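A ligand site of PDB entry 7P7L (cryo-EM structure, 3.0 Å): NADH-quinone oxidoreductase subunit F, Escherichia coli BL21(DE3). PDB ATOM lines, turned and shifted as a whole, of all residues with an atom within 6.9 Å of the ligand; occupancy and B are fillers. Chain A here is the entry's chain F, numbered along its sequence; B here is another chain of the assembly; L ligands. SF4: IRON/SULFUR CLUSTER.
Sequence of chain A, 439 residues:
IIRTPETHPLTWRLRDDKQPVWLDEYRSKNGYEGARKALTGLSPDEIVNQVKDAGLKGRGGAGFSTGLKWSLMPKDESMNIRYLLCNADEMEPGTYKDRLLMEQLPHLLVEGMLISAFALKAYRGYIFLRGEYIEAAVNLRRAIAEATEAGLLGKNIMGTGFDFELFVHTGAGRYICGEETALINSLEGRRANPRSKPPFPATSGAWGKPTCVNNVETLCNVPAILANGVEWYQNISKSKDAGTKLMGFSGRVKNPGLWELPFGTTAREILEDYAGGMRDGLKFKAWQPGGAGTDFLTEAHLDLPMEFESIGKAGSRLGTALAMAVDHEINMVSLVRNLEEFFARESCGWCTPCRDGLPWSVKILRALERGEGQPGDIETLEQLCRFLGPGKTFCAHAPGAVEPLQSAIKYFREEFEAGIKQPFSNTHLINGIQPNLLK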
ATOM      1  N   ILE A 176      -5.281   9.897   6.183  1.00  0.00           N
ATOM      2  CA  ILE A 176      -5.537  10.991   5.260  1.00  0.00           C
ATOM      3  C   ILE A 176      -5.620  12.347   5.947  1.00  0.00           C
ATOM      4  O   ILE A 176      -5.561  13.375   5.268  1.00  0.00           O
ATOM      5  CB  ILE A 176      -6.820  10.701   4.444  1.00  0.00           C
ATOM      6  CG1 ILE A 176      -6.756  11.367   3.071  1.00  0.00           C
ATOM      7  CG2 ILE A 176      -8.062  11.135   5.209  1.00  0.00           C
ATOM      8  CD1 ILE A 176      -5.489  11.070   2.298  1.00  0.00           C
ATOM      9  N   ALA A 192     -12.548  14.172   6.884  1.00  0.00           N
ATOM     10  CA  ALA A 192     -11.267  14.650   6.366  1.00  0.00           C
ATOM     11  C   ALA A 192     -11.144  14.315   4.882  1.00  0.00           C
ATOM     12  O   ALA A 192     -10.460  13.376   4.462  1.00  0.00           O
ATOM     13  CB  ALA A 192     -10.119  14.053   7.176  1.00  0.00           C
ATOM     14  N   ASN A 193     -11.823  15.112   4.077  1.00  0.00           N
ATOM     15  CA  ASN A 193     -11.734  15.017   2.629  1.00  0.00           C
ATOM     16  C   ASN A 193     -10.869  16.140   2.098  1.00  0.00           C
ATOM     17  O   ASN A 193     -11.025  17.288   2.548  1.00  0.00           O
ATOM     18  CB  ASN A 193     -13.116  15.086   1.990  1.00  0.00           C
ATOM     19  CG  ASN A 193     -14.045  14.010   2.488  1.00  0.00           C
ATOM     20  OD1 ASN A 193     -15.112  14.295   3.044  1.00  0.00           O
ATOM     21  ND2 ASN A 193     -13.650  12.757   2.306  1.00  0.00           N
ATOM     22  N   PRO A 194      -9.948  15.872   1.186  1.00  0.00           N
ATOM     23  CA  PRO A 194      -9.121  16.945   0.636  1.00  0.00           C
ATOM     24  C   PRO A 194      -9.916  17.866  -0.269  1.00  0.00           C
ATOM     25  O   PRO A 194     -11.010  17.536  -0.738  1.00  0.00           O
ATOM     26  CB  PRO A 194      -8.037  16.198  -0.146  1.00  0.00           C
ATOM     27  CG  PRO A 194      -8.665  14.903  -0.510  1.00  0.00           C
ATOM     28  CD  PRO A 194      -9.596  14.560   0.625  1.00  0.00           C
ATOM     29  N   PHE A 343      -2.630   1.359   2.709  1.00  0.00           N
ATOM     30  CA  PHE A 343      -3.049   2.503   1.911  1.00  0.00           C
ATOM     31  C   PHE A 343      -4.492   2.391   1.445  1.00  0.00           C
ATOM     32  O   PHE A 343      -5.104   3.416   1.112  1.00  0.00           O
ATOM     33  CB  PHE A 343      -2.131   2.670   0.703  1.00  0.00           C
ATOM     34  CG  PHE A 343      -0.908   3.487   0.994  1.00  0.00           C
ATOM     35  CD1 PHE A 343      -1.015   4.842   1.263  1.00  0.00           C
ATOM     36  CD2 PHE A 343       0.354   2.910   0.993  1.00  0.00           C
ATOM     37  CE1 PHE A 343       0.107   5.589   1.538  1.00  0.00           C
ATOM     38  CE2 PHE A 343       1.476   3.658   1.268  1.00  0.00           C
ATOM     39  CZ  PHE A 343       1.357   5.006   1.537  1.00  0.00           C
ATOM     40  N   GLU A 346      -6.794   2.889   4.858  1.00  0.00           N
ATOM     41  CA  GLU A 346      -6.656   4.239   5.390  1.00  0.00           C
ATOM     42  C   GLU A 346      -6.833   5.306   4.316  1.00  0.00           C
ATOM     43  O   GLU A 346      -6.543   6.475   4.567  1.00  0.00           O
ATOM     44  CB  GLU A 346      -5.301   4.407   6.069  1.00  0.00           C
ATOM     45  CG  GLU A 346      -5.135   3.543   7.312  1.00  0.00           C
ATOM     46  CD  GLU A 346      -5.887   4.078   8.505  1.00  0.00           C
ATOM     47  OE1 GLU A 346      -6.087   5.309   8.579  1.00  0.00           O
ATOM     48  OE2 GLU A 346      -6.291   3.270   9.363  1.00  0.00           O
ATOM     49  N   SER A 347      -7.303   4.926   3.129  1.00  0.00           N
ATOM     50  CA  SER A 347      -7.661   5.927   2.132  1.00  0.00           C
ATOM     51  C   SER A 347      -8.963   6.617   2.530  1.00  0.00           C
ATOM     52  O   SER A 347      -9.747   6.119   3.333  1.00  0.00           O
ATOM     53  CB  SER A 347      -7.814   5.274   0.750  1.00  0.00           C
ATOM     54  OG  SER A 347      -8.157   6.243  -0.225  1.00  0.00           O
ATOM     55  N   CYS A 348      -9.178   7.790   1.951  1.00  0.00           N
ATOM     56  CA  CYS A 348     -10.364   8.566   2.254  1.00  0.00           C
ATOM     57  C   CYS A 348     -11.575   8.165   1.413  1.00  0.00           C
ATOM     58  O   CYS A 348     -12.711   8.419   1.825  1.00  0.00           O
ATOM     59  CB  CYS A 348     -10.089  10.058   2.068  1.00  0.00           C
ATOM     60  SG  CYS A 348     -10.705  10.694   0.524  1.00  0.00           S
ATOM     61  N   GLY A 349     -11.349   7.540   0.256  1.00  0.00           N
ATOM     62  CA  GLY A 349     -12.450   7.016  -0.520  1.00  0.00           C
ATOM     63  C   GLY A 349     -13.263   8.045  -1.267  1.00  0.00           C
ATOM     64  O   GLY A 349     -14.423   7.777  -1.600  1.00  0.00           O
ATOM     65  N   TRP A 350     -12.704   9.215  -1.548  1.00  0.00           N
ATOM     66  CA  TRP A 350     -13.449  10.234  -2.280  1.00  0.00           C
ATOM     67  C   TRP A 350     -13.557   9.871  -3.758  1.00  0.00           C
ATOM     68  O   TRP A 350     -14.653   9.734  -4.297  1.00  0.00           O
ATOM     69  CB  TRP A 350     -12.794  11.608  -2.116  1.00  0.00           C
ATOM     70  CG  TRP A 350     -13.435  12.689  -2.898  1.00  0.00           C
ATOM     71  CD1 TRP A 350     -12.999  13.225  -4.070  1.00  0.00           C
ATOM     72  CD2 TRP A 350     -14.652  13.370  -2.576  1.00  0.00           C
ATOM     73  NE1 TRP A 350     -13.861  14.200  -4.495  1.00  0.00           N
ATOM     74  CE2 TRP A 350     -14.885  14.312  -3.587  1.00  0.00           C
ATOM     75  CE3 TRP A 350     -15.556  13.273  -1.520  1.00  0.00           C
ATOM     76  CZ2 TRP A 350     -15.984  15.161  -3.579  1.00  0.00           C
ATOM     77  CZ3 TRP A 350     -16.658  14.112  -1.508  1.00  0.00           C
ATOM     78  CH2 TRP A 350     -16.863  15.045  -2.541  1.00  0.00           C
ATOM     79  N   CYS A 351     -12.417   9.709  -4.418  1.00  0.00           N
ATOM     80  CA  CYS A 351     -12.406   9.625  -5.859  1.00  0.00           C
ATOM     81  C   CYS A 351     -12.212   8.201  -6.348  1.00  0.00           C
ATOM     82  O   CYS A 351     -11.553   7.385  -5.691  1.00  0.00           O
ATOM     83  CB  CYS A 351     -11.339  10.557  -6.451  1.00  0.00           C
ATOM     84  SG  CYS A 351      -9.631  10.094  -6.231  1.00  0.00           S
ATOM     85  N   THR A 352     -12.798   7.923  -7.518  1.00  0.00           N
ATOM     86  CA  THR A 352     -12.968   6.559  -8.004  1.00  0.00           C
ATOM     87  C   THR A 352     -11.686   5.746  -8.189  1.00  0.00           C
ATOM     88  O   THR A 352     -11.679   4.580  -7.745  1.00  0.00           O
ATOM     89  CB  THR A 352     -13.774   6.595  -9.314  1.00  0.00           C
ATOM     90  OG1 THR A 352     -15.091   7.098  -9.043  1.00  0.00           O
ATOM     91  CG2 THR A 352     -13.886   5.214  -9.950  1.00  0.00           C
ATOM     92  N   PRO A 353     -10.603   6.241  -8.809  1.00  0.00           N
ATOM     93  CA  PRO A 353      -9.478   5.335  -9.095  1.00  0.00           C
ATOM     94  C   PRO A 353      -8.817   4.745  -7.868  1.00  0.00           C
ATOM     95  O   PRO A 353      -8.668   3.516  -7.795  1.00  0.00           O
ATOM     96  CB  PRO A 353      -8.513   6.224  -9.893  1.00  0.00           C
ATOM     97  CG  PRO A 353      -9.346   7.269 -10.453  1.00  0.00           C
ATOM     98  CD  PRO A 353     -10.306   7.577  -9.374  1.00  0.00           C
ATOM     99  N   CYS A 354      -8.451   5.554  -6.872  1.00  0.00           N
ATOM    100  CA  CYS A 354      -7.849   5.018  -5.657  1.00  0.00           C
ATOM    101  C   CYS A 354      -8.849   4.153  -4.894  1.00  0.00           C
ATOM    102  O   CYS A 354      -8.547   3.003  -4.561  1.00  0.00           O
ATOM    103  CB  CYS A 354      -7.310   6.160  -4.802  1.00  0.00           C
ATOM    104  SG  CYS A 354      -7.332   6.022  -2.986  1.00  0.00           S
ATOM    105  N   ARG A 355     -10.081   4.649  -4.723  1.00  0.00           N
ATOM    106  CA  ARG A 355     -11.083   3.973  -3.899  1.00  0.00           C
ATOM    107  C   ARG A 355     -11.464   2.603  -4.444  1.00  0.00           C
ATOM    108  O   ARG A 355     -11.660   1.655  -3.684  1.00  0.00           O
ATOM    109  CB  ARG A 355     -12.331   4.860  -3.780  1.00  0.00           C
ATOM    110  CG  ARG A 355     -13.490   4.214  -3.041  1.00  0.00           C
ATOM    111  CD  ARG A 355     -14.803   4.945  -3.279  1.00  0.00           C
ATOM    112  NE  ARG A 355     -15.312   4.758  -4.629  1.00  0.00           N
ATOM    113  CZ  ARG A 355     -15.497   5.741  -5.495  1.00  0.00           C
ATOM    114  NH1 ARG A 355     -15.265   7.006  -5.183  1.00  0.00           N
ATOM    115  NH2 ARG A 355     -15.942   5.454  -6.713  1.00  0.00           N
ATOM    116  N   LEU A 358      -7.343   0.449  -5.458  1.00  0.00           N
ATOM    117  CA  LEU A 358      -6.499  -0.089  -4.394  1.00  0.00           C
ATOM    118  C   LEU A 358      -7.019  -1.409  -3.821  1.00  0.00           C
ATOM    119  O   LEU A 358      -6.176  -2.279  -3.551  1.00  0.00           O
ATOM    120  CB  LEU A 358      -6.303   0.971  -3.302  1.00  0.00           C
ATOM    121  CG  LEU A 358      -5.359   2.122  -3.660  1.00  0.00           C
ATOM    122  CD1 LEU A 358      -5.085   2.978  -2.447  1.00  0.00           C
ATOM    123  CD2 LEU A 358      -4.058   1.580  -4.233  1.00  0.00           C
ATOM    124  N   LEU A 388      -2.959   6.179 -11.817  1.00  0.00           N
ATOM    125  CA  LEU A 388      -3.035   6.690 -10.449  1.00  0.00           C
ATOM    126  C   LEU A 388      -1.953   7.736 -10.195  1.00  0.00           C
ATOM    127  O   LEU A 388      -1.543   7.907  -9.041  1.00  0.00           O
ATOM    128  CB  LEU A 388      -2.904   5.559  -9.436  1.00  0.00           C
ATOM    129  CG  LEU A 388      -3.851   5.572  -8.241  1.00  0.00           C
ATOM    130  CD1 LEU A 388      -5.252   5.314  -8.709  1.00  0.00           C
ATOM    131  CD2 LEU A 388      -3.466   4.519  -7.231  1.00  0.00           C
ATOM    132  N   THR A 393      -5.511  11.204  -9.784  1.00  0.00           N
ATOM    133  CA  THR A 393      -6.441  11.108  -8.666  1.00  0.00           C
ATOM    134  C   THR A 393      -6.755  12.502  -8.149  1.00  0.00           C
ATOM    135  O   THR A 393      -6.243  13.508  -8.648  1.00  0.00           O
ATOM    136  CB  THR A 393      -5.857  10.221  -7.558  1.00  0.00           C
ATOM    137  OG1 THR A 393      -4.833  10.946  -6.854  1.00  0.00           O
ATOM    138  CG2 THR A 393      -5.246   8.979  -8.165  1.00  0.00           C
ATOM    139  N   PHE A 394      -7.614  12.567  -7.132  1.00  0.00           N
ATOM    140  CA  PHE A 394      -7.998  13.864  -6.583  1.00  0.00           C
ATOM    141  C   PHE A 394      -6.859  14.519  -5.819  1.00  0.00           C
ATOM    142  O   PHE A 394      -6.746  15.747  -5.827  1.00  0.00           O
ATOM    143  CB  PHE A 394      -9.220  13.681  -5.691  1.00  0.00           C
ATOM    144  CG  PHE A 394      -9.868  14.969  -5.261  1.00  0.00           C
ATOM    145  CD1 PHE A 394     -10.824  15.580  -6.069  1.00  0.00           C
ATOM    146  CD2 PHE A 394      -9.541  15.567  -4.057  1.00  0.00           C
ATOM    147  CE1 PHE A 394     -11.429  16.755  -5.671  1.00  0.00           C
ATOM    148  CE2 PHE A 394     -10.131  16.745  -3.668  1.00  0.00           C
ATOM    149  CZ  PHE A 394     -11.079  17.340  -4.477  1.00  0.00           C
ATOM    150  N   CYS A 395      -6.014  13.727  -5.168  1.00  0.00           N
ATOM    151  CA  CYS A 395      -4.886  14.261  -4.424  1.00  0.00           C
ATOM    152  C   CYS A 395      -3.675  13.356  -4.650  1.00  0.00           C
ATOM    153  O   CYS A 395      -3.685  12.500  -5.540  1.00  0.00           O
ATOM    154  CB  CYS A 395      -5.223  14.409  -2.936  1.00  0.00           C
ATOM    155  SG  CYS A 395      -4.759  12.981  -1.936  1.00  0.00           S
ATOM    156  N   ALA A 396      -2.642  13.544  -3.829  1.00  0.00           N
ATOM    157  CA  ALA A 396      -1.381  12.849  -4.001  1.00  0.00           C
ATOM    158  C   ALA A 396      -1.203  11.675  -3.045  1.00  0.00           C
ATOM    159  O   ALA A 396      -0.086  11.146  -2.939  1.00  0.00           O
ATOM    160  CB  ALA A 396      -0.220  13.839  -3.834  1.00  0.00           C
ATOM    161  N   HIS A 397      -2.256  11.274  -2.338  1.00  0.00           N
ATOM    162  CA  HIS A 397      -2.155  10.111  -1.457  1.00  0.00           C
ATOM    163  C   HIS A 397      -1.963   8.825  -2.256  1.00  0.00           C
ATOM    164  O   HIS A 397      -1.163   7.959  -1.883  1.00  0.00           O
ATOM    165  CB  HIS A 397      -3.390  10.000  -0.572  1.00  0.00           C
ATOM    166  CG  HIS A 397      -3.700   8.600  -0.118  1.00  0.00           C
ATOM    167  ND1 HIS A 397      -4.592   7.786  -0.794  1.00  0.00           N
ATOM    168  CD2 HIS A 397      -3.261   7.890   0.934  1.00  0.00           C
ATOM    169  CE1 HIS A 397      -4.669   6.623  -0.177  1.00  0.00           C
ATOM    170  NE2 HIS A 397      -3.871   6.660   0.880  1.00  0.00           N
ATOM    171  N   ALA A 398      -2.681   8.697  -3.369  1.00  0.00           N
ATOM    172  CA  ALA A 398      -2.622   7.501  -4.196  1.00  0.00           C
ATOM    173  C   ALA A 398      -1.362   7.376  -5.064  1.00  0.00           C
ATOM    174  O   ALA A 398      -0.881   6.251  -5.243  1.00  0.00           O
ATOM    175  CB  ALA A 398      -3.890   7.417  -5.060  1.00  0.00           C
ATOM    176  N   PRO A 399      -0.806   8.469  -5.645  1.00  0.00           N
ATOM    177  CA  PRO A 399       0.551   8.333  -6.221  1.00  0.00           C
ATOM    178  C   PRO A 399       1.594   7.858  -5.226  1.00  0.00           C
ATOM    179  O   PRO A 399       2.425   7.000  -5.553  1.00  0.00           O
ATOM    180  CB  PRO A 399       0.852   9.752  -6.723  1.00  0.00           C
ATOM    181  CG  PRO A 399      -0.453  10.299  -7.059  1.00  0.00           C
ATOM    182  CD  PRO A 399      -1.420   9.752  -6.059  1.00  0.00           C
ATOM    183  N   ALA B  43     -15.476  13.873  -8.180  1.00  0.00           N
ATOM    184  CA  ALA B  43     -15.285  12.620  -7.483  1.00  0.00           C
ATOM    185  C   ALA B  43     -15.137  11.440  -8.433  1.00  0.00           C
ATOM    186  O   ALA B  43     -14.174  10.684  -8.331  1.00  0.00           O
ATOM    187  CB  ALA B  43     -16.445  12.373  -6.514  1.00  0.00           C
ATOM    188  N   ARG B  45     -14.248  10.881 -11.439  1.00  0.00           N
ATOM    189  CA  ARG B  45     -13.057  10.798 -12.303  1.00  0.00           C
ATOM    190  C   ARG B  45     -13.381  10.248 -13.695  1.00  0.00           C
ATOM    191  O   ARG B  45     -12.571   9.549 -14.302  1.00  0.00           O
ATOM    192  CB  ARG B  45     -11.954   9.967 -11.626  1.00  0.00           C
ATOM    193  CG  ARG B  45     -10.523  10.346 -11.977  1.00  0.00           C
ATOM    194  CD  ARG B  45     -10.119  11.686 -11.398  1.00  0.00           C
ATOM    195  NE  ARG B  45     -10.732  11.960 -10.106  1.00  0.00           N
ATOM    196  CZ  ARG B  45     -10.667  13.138  -9.503  1.00  0.00           C
ATOM    197  NH1 ARG B  45     -10.031  14.165 -10.048  1.00  0.00           N
ATOM    198  NH2 ARG B  45     -11.259  13.296  -8.329  1.00  0.00           N
ATOM    199  N   HIS B 175     -12.893   4.682   2.711  1.00  0.00           N
ATOM    200  CA  HIS B 175     -12.478   3.936   1.510  1.00  0.00           C
ATOM    201  C   HIS B 175     -13.648   3.486   0.650  1.00  0.00           C
ATOM    202  O   HIS B 175     -14.484   4.316   0.263  1.00  0.00           O
ATOM    203  CB  HIS B 175     -11.580   2.737   1.880  1.00  0.00           C
ATOM    204  CG  HIS B 175     -11.953   2.012   3.136  1.00  0.00           C
ATOM    205  ND1 HIS B 175     -11.479   2.398   4.369  1.00  0.00           N
ATOM    206  CD2 HIS B 175     -12.743   0.937   3.358  1.00  0.00           C
ATOM    207  CE1 HIS B 175     -11.970   1.586   5.298  1.00  0.00           C
ATOM    208  NE2 HIS B 175     -12.736   0.693   4.701  1.00  0.00           N
HETATM  209 FE1  SF4 L   1      -8.929  10.063  -4.015  1.00  0.00          FE
HETATM  210 FE2  SF4 L   1      -7.797   8.243  -2.503  1.00  0.00          FE
HETATM  211 FE3  SF4 L   1      -6.970  10.851  -2.274  1.00  0.00          FE
HETATM  212 FE4  SF4 L   1      -9.306  10.122  -1.247  1.00  0.00          FE
HETATM  213  S1  SF4 L   1      -7.252   9.340  -0.555  1.00  0.00           S
HETATM  214  S2  SF4 L   1      -8.976  11.920  -2.650  1.00  0.00           S
HETATM  215  S3  SF4 L   1     -10.074   8.546  -2.732  1.00  0.00           S
HETATM  216  S4  SF4 L   1      -6.709   9.493  -4.093  1.00  0.00           S
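The side-chain sulfur of Cys 348 binds an iron atom (FE4) of the ligand (2.3 Å).
A ring nitrogen (ND1) of His 397 lies close to a sulfur (S1) of the ligand, 3.1 Å away.
A sulfur (S1) of the ligand lies close to the side-chain hydroxyl (OG) of Ser 347, 3.2 Å away.
N of Cys 351 lies close to S3 of the ligand.
The side-chain sulfur (SG) of Cys 354 is bound to an iron atom (FE2) of the ligand, 2.3 Å away.
N of Trp 350 sits close to S3 of the ligand.
The backbone NH (N) of Gly 349 sits close to a sulfur (S3) of the ligand (3.4 Å).
FE1 of the ligand is bound by SG of Cys 351, 2.3 Å away.
The backbone NH of Cys 348 lies close to a sulfur (S1) of the ligand (3.5 Å).
The side-chain hydroxyl (OG1) of Thr 393 sits close to a sulfur (S4) of the ligand.
The side-chain sulfur of Cys 351 sits close to the backbone NH of Phe 394.
OG of Ser 347 lies close to N of Gly 349.
SG of Cys 348 sits close to N of Trp 350, 3.2 Å away.
The backbone NH (N) of Cys 395 sits close to the side-chain hydroxyl (OG1) of Thr 393, at 3.5 Å.
The backbone carbonyl oxygen of Trp 350 is in hydrogen-bond range of the guanidinium group of Arg 355, 2.9 Å away.
The side-chain sulfur of Cys 354 sits close to the side-chain hydroxyl of Ser 347, at 2.9 Å.
A ring nitrogen (NE2) of His 397 sits close to the backbone carbonyl oxygen of Phe 343 (3.5 Å).
The side-chain sulfur of Cys 395 lies within hydrogen-bond range of the backbone NH of His 397, at 3.1 Å.
Ile 176 touches the ligand.
CG of Pro 194 touches S2 of the ligand, 3.7 Å away.
CB of Phe 394 touches S2 of the ligand, at 3.5 Å.
SG of Cys 395 touches FE3 of the ligand (3.1 Å).
CB of Ala 398 touches S4 of the ligand, 3.6 Å away.
Hydrophobic or aromatic side chains that line the ligand: Ile 176, Pro 194, Trp 350, Phe 394, His 397 and Ala 398.
The nearest printed residue that does not touch the ligand is Arg 355 (4.4 Å).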
